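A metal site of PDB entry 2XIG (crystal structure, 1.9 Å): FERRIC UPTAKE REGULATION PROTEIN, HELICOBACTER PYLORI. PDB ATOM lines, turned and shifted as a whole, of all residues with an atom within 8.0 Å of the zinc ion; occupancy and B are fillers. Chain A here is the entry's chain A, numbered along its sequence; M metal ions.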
ATOM      1  N   HIS A  96      18.750 -15.863  26.133  1.00  0.00           N
ATOM      2  CA  HIS A  96      19.100 -14.458  26.029  1.00  0.00           C
ATOM      3  C   HIS A  96      20.502 -14.269  25.472  1.00  0.00           C
ATOM      4  O   HIS A  96      21.437 -14.998  25.811  1.00  0.00           O
ATOM      5  CB  HIS A  96      19.030 -13.763  27.389  1.00  0.00           C
ATOM      6  CG  HIS A  96      19.630 -12.403  27.372  1.00  0.00           C
ATOM      7  ND1 HIS A  96      18.993 -11.319  26.795  1.00  0.00           N
ATOM      8  CD2 HIS A  96      20.845 -11.956  27.778  1.00  0.00           C
ATOM      9  CE1 HIS A  96      19.781 -10.261  26.881  1.00  0.00           C
ATOM     10  NE2 HIS A  96      20.910 -10.616  27.470  1.00  0.00           N
ATOM     11  N   HIS A  97      20.649 -13.275  24.610  1.00  0.00           N
ATOM     12  CA  HIS A  97      21.964 -12.908  24.129  1.00  0.00           C
ATOM     13  C   HIS A  97      21.947 -11.481  23.634  1.00  0.00           C
ATOM     14  O   HIS A  97      20.884 -10.941  23.313  1.00  0.00           O
ATOM     15  CB  HIS A  97      22.412 -13.841  23.003  1.00  0.00           C
ATOM     16  CG  HIS A  97      21.561 -13.753  21.785  1.00  0.00           C
ATOM     17  ND1 HIS A  97      20.354 -14.408  21.662  1.00  0.00           N
ATOM     18  CD2 HIS A  97      21.737 -13.061  20.631  1.00  0.00           C
ATOM     19  CE1 HIS A  97      19.834 -14.127  20.475  1.00  0.00           C
ATOM     20  NE2 HIS A  97      20.653 -13.329  19.828  1.00  0.00           N
ATOM     21  N   ASP A  98      23.120 -10.886  23.559  1.00  0.00           N
ATOM     22  CA  ASP A  98      23.251  -9.538  23.020  1.00  0.00           C
ATOM     23  C   ASP A  98      24.035  -9.601  21.716  1.00  0.00           C
ATOM     24  O   ASP A  98      24.428 -10.676  21.275  1.00  0.00           O
ATOM     25  CB  ASP A  98      23.925  -8.643  24.047  1.00  0.00           C
ATOM     26  CG  ASP A  98      23.211  -8.674  25.393  1.00  0.00           C
ATOM     27  OD1 ASP A  98      22.084  -8.144  25.495  1.00  0.00           O
ATOM     28  OD2 ASP A  98      23.775  -9.238  26.349  1.00  0.00           O
ATOM     29  N   HIS A  99      24.249  -8.454  21.074  1.00  0.00           N
ATOM     30  CA  HIS A  99      24.829  -8.456  19.736  1.00  0.00           C
ATOM     31  C   HIS A  99      26.004  -7.530  19.557  1.00  0.00           C
ATOM     32  O   HIS A  99      26.013  -6.407  20.036  1.00  0.00           O
ATOM     33  CB  HIS A  99      23.778  -8.104  18.674  1.00  0.00           C
ATOM     34  CG  HIS A  99      22.584  -8.993  18.714  1.00  0.00           C
ATOM     35  ND1 HIS A  99      21.525  -8.772  19.560  1.00  0.00           N
ATOM     36  CD2 HIS A  99      22.290 -10.130  18.033  1.00  0.00           C
ATOM     37  CE1 HIS A  99      20.617  -9.715  19.398  1.00  0.00           C
ATOM     38  NE2 HIS A  99      21.060 -10.557  18.471  1.00  0.00           N
ATOM     39  N   PHE A 111      26.497 -12.879  21.692  1.00  0.00           N
ATOM     40  CA  PHE A 111      27.229 -13.142  22.933  1.00  0.00           C
ATOM     41  C   PHE A 111      26.325 -13.010  24.131  1.00  0.00           C
ATOM     42  O   PHE A 111      25.284 -12.337  24.089  1.00  0.00           O
ATOM     43  CB  PHE A 111      28.449 -12.209  23.069  1.00  0.00           C
ATOM     44  CG  PHE A 111      28.100 -10.775  23.417  1.00  0.00           C
ATOM     45  CD1 PHE A 111      27.765  -9.860  22.425  1.00  0.00           C
ATOM     46  CD2 PHE A 111      28.101 -10.338  24.738  1.00  0.00           C
ATOM     47  CE1 PHE A 111      27.448  -8.540  22.733  1.00  0.00           C
ATOM     48  CE2 PHE A 111      27.782  -9.030  25.065  1.00  0.00           C
ATOM     49  CZ  PHE A 111      27.460  -8.125  24.057  1.00  0.00           C
ATOM     50  N   ALA A 112      26.724 -13.657  25.216  1.00  0.00           N
ATOM     51  CA  ALA A 112      26.033 -13.540  26.484  1.00  0.00           C
ATOM     52  C   ALA A 112      27.068 -13.701  27.596  1.00  0.00           C
ATOM     53  O   ALA A 112      27.534 -14.806  27.841  1.00  0.00           O
ATOM     54  CB  ALA A 112      24.948 -14.586  26.598  1.00  0.00           C
ATOM     55  N   ASP A 113      27.424 -12.595  28.231  1.00  0.00           N
ATOM     56  CA  ASP A 113      28.495 -12.571  29.215  1.00  0.00           C
ATOM     57  C   ASP A 113      27.926 -12.526  30.636  1.00  0.00           C
ATOM     58  O   ASP A 113      27.383 -11.500  31.057  1.00  0.00           O
ATOM     59  CB  ASP A 113      29.393 -11.353  28.982  1.00  0.00           C
ATOM     60  CG  ASP A 113      30.678 -11.413  29.775  1.00  0.00           C
ATOM     61  OD1 ASP A 113      31.523 -12.284  29.486  1.00  0.00           O
ATOM     62  OD2 ASP A 113      30.854 -10.580  30.692  1.00  0.00           O
ATOM     63  N   ILE A 116      28.762  -9.423  32.711  1.00  0.00           N
ATOM     64  CA  ILE A 116      28.054  -8.226  32.288  1.00  0.00           C
ATOM     65  C   ILE A 116      26.620  -8.254  32.803  1.00  0.00           C
ATOM     66  O   ILE A 116      26.115  -7.255  33.322  1.00  0.00           O
ATOM     67  CB  ILE A 116      28.052  -8.070  30.767  1.00  0.00           C
ATOM     68  CG1 ILE A 116      29.468  -7.747  30.272  1.00  0.00           C
ATOM     69  CG2 ILE A 116      27.050  -7.011  30.332  1.00  0.00           C
ATOM     70  CD1 ILE A 116      29.528  -7.318  28.831  1.00  0.00           C
ATOM     71  N   GLU A 117      25.953  -9.398  32.645  1.00  0.00           N
ATOM     72  CA  GLU A 117      24.576  -9.528  33.104  1.00  0.00           C
ATOM     73  C   GLU A 117      24.493  -9.301  34.617  1.00  0.00           C
ATOM     74  O   GLU A 117      23.569  -8.655  35.105  1.00  0.00           O
ATOM     75  CB  GLU A 117      24.015 -10.906  32.748  1.00  0.00           C
ATOM     76  CG  GLU A 117      24.129 -11.273  31.281  1.00  0.00           C
ATOM     77  CD  GLU A 117      23.239 -10.446  30.381  1.00  0.00           C
ATOM     78  OE1 GLU A 117      22.108 -10.099  30.797  1.00  0.00           O
ATOM     79  OE2 GLU A 117      23.662 -10.161  29.239  1.00  0.00           O
ATOM     80  N   GLN A 120      25.048  -5.537  35.472  1.00  0.00           N
ATOM     81  CA  GLN A 120      23.871  -4.732  35.148  1.00  0.00           C
ATOM     82  C   GLN A 120      22.881  -4.762  36.312  1.00  0.00           C
ATOM     83  O   GLN A 120      22.200  -3.776  36.586  1.00  0.00           O
ATOM     84  CB  GLN A 120      23.176  -5.265  33.885  1.00  0.00           C
ATOM     85  CG  GLN A 120      23.960  -5.056  32.594  1.00  0.00           C
ATOM     86  CD  GLN A 120      23.316  -5.757  31.397  1.00  0.00           C
ATOM     87  OE1 GLN A 120      22.411  -6.576  31.555  1.00  0.00           O
ATOM     88  NE2 GLN A 120      23.790  -5.430  30.207  1.00  0.00           N
ATOM     89  N   SER A 133      14.296  -5.488  31.611  1.00  0.00           N
ATOM     90  CA  SER A 133      14.972  -5.988  30.416  1.00  0.00           C
ATOM     91  C   SER A 133      16.068  -5.030  29.998  1.00  0.00           C
ATOM     92  O   SER A 133      16.193  -3.936  30.554  1.00  0.00           O
ATOM     93  CB  SER A 133      13.982  -6.162  29.265  1.00  0.00           C
ATOM     94  OG  SER A 133      13.544  -4.889  28.789  1.00  0.00           O
ATOM     95  N   HIS A 134      16.850  -5.425  29.006  1.00  0.00           N
ATOM     96  CA  HIS A 134      17.850  -4.513  28.484  1.00  0.00           C
ATOM     97  C   HIS A 134      18.082  -4.753  27.009  1.00  0.00           C
ATOM     98  O   HIS A 134      17.631  -5.747  26.444  1.00  0.00           O
ATOM     99  CB  HIS A 134      19.156  -4.633  29.267  1.00  0.00           C
ATOM    100  CG  HIS A 134      19.778  -5.978  29.202  1.00  0.00           C
ATOM    101  ND1 HIS A 134      19.348  -7.039  29.987  1.00  0.00           N
ATOM    102  CD2 HIS A 134      20.776  -6.474  28.422  1.00  0.00           C
ATOM    103  CE1 HIS A 134      20.061  -8.106  29.706  1.00  0.00           C
ATOM    104  NE2 HIS A 134      20.939  -7.798  28.763  1.00  0.00           N
ATOM    105  N   ASP A 135      18.793  -3.832  26.384  1.00  0.00           N
ATOM    106  CA  ASP A 135      19.148  -4.001  24.995  1.00  0.00           C
ATOM    107  C   ASP A 135      20.570  -3.465  24.862  1.00  0.00           C
ATOM    108  O   ASP A 135      20.851  -2.336  25.236  1.00  0.00           O
ATOM    109  CB  ASP A 135      18.171  -3.238  24.109  1.00  0.00           C
ATOM    110  CG  ASP A 135      18.441  -3.460  22.634  1.00  0.00           C
ATOM    111  OD1 ASP A 135      19.467  -2.968  22.133  1.00  0.00           O
ATOM    112  OD2 ASP A 135      17.614  -4.137  21.979  1.00  0.00           O
ATOM    113  N   MET A 136      21.466  -4.328  24.395  1.00  0.00           N
ATOM    114  CA  MET A 136      22.886  -3.995  24.364  1.00  0.00           C
ATOM    115  C   MET A 136      23.425  -4.347  22.985  1.00  0.00           C
ATOM    116  O   MET A 136      23.334  -5.494  22.563  1.00  0.00           O
ATOM    117  CB  MET A 136      23.647  -4.751  25.459  1.00  0.00           C
ATOM    118  CG  MET A 136      25.173  -4.668  25.361  1.00  0.00           C
ATOM    119  SD  MET A 136      25.975  -5.520  26.729  1.00  0.00           S
ATOM    120  CE  MET A 136      27.668  -5.570  26.193  1.00  0.00           C
HETATM  121 ZN    ZN M   1      22.332  -9.163  27.894  1.00  0.00          ZN
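Within 4 Å of the zinc ion: His 96, Asp 98, Glu 117 and His 134. The nearest printed residue that does not touch the zinc ion is Gln 120 (4.5 Å).
The backbone carbonyl oxygen (O) of Phe 111 lies within hydrogen-bond range of the backbone NH (N) of Asp 98 (2.7 Å). A ring nitrogen (ND1) of His 134 lies close to the side-chain amide oxygen of Gln 120.
The zinc ion is bound by a ring nitrogen (NE2) of His 96 (2.1 Å), the side-chain carboxylate (OD2) of Asp 98 (2.1 Å), a ring nitrogen (NE2) of His 134 (2.1 Å) and the side-chain carboxylate (OE2) of Glu 117 (2.1 Å). Slightly farther from the zinc ion lies the side-chain carboxylate (OD1) of Asp 98 (2.6 Å).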
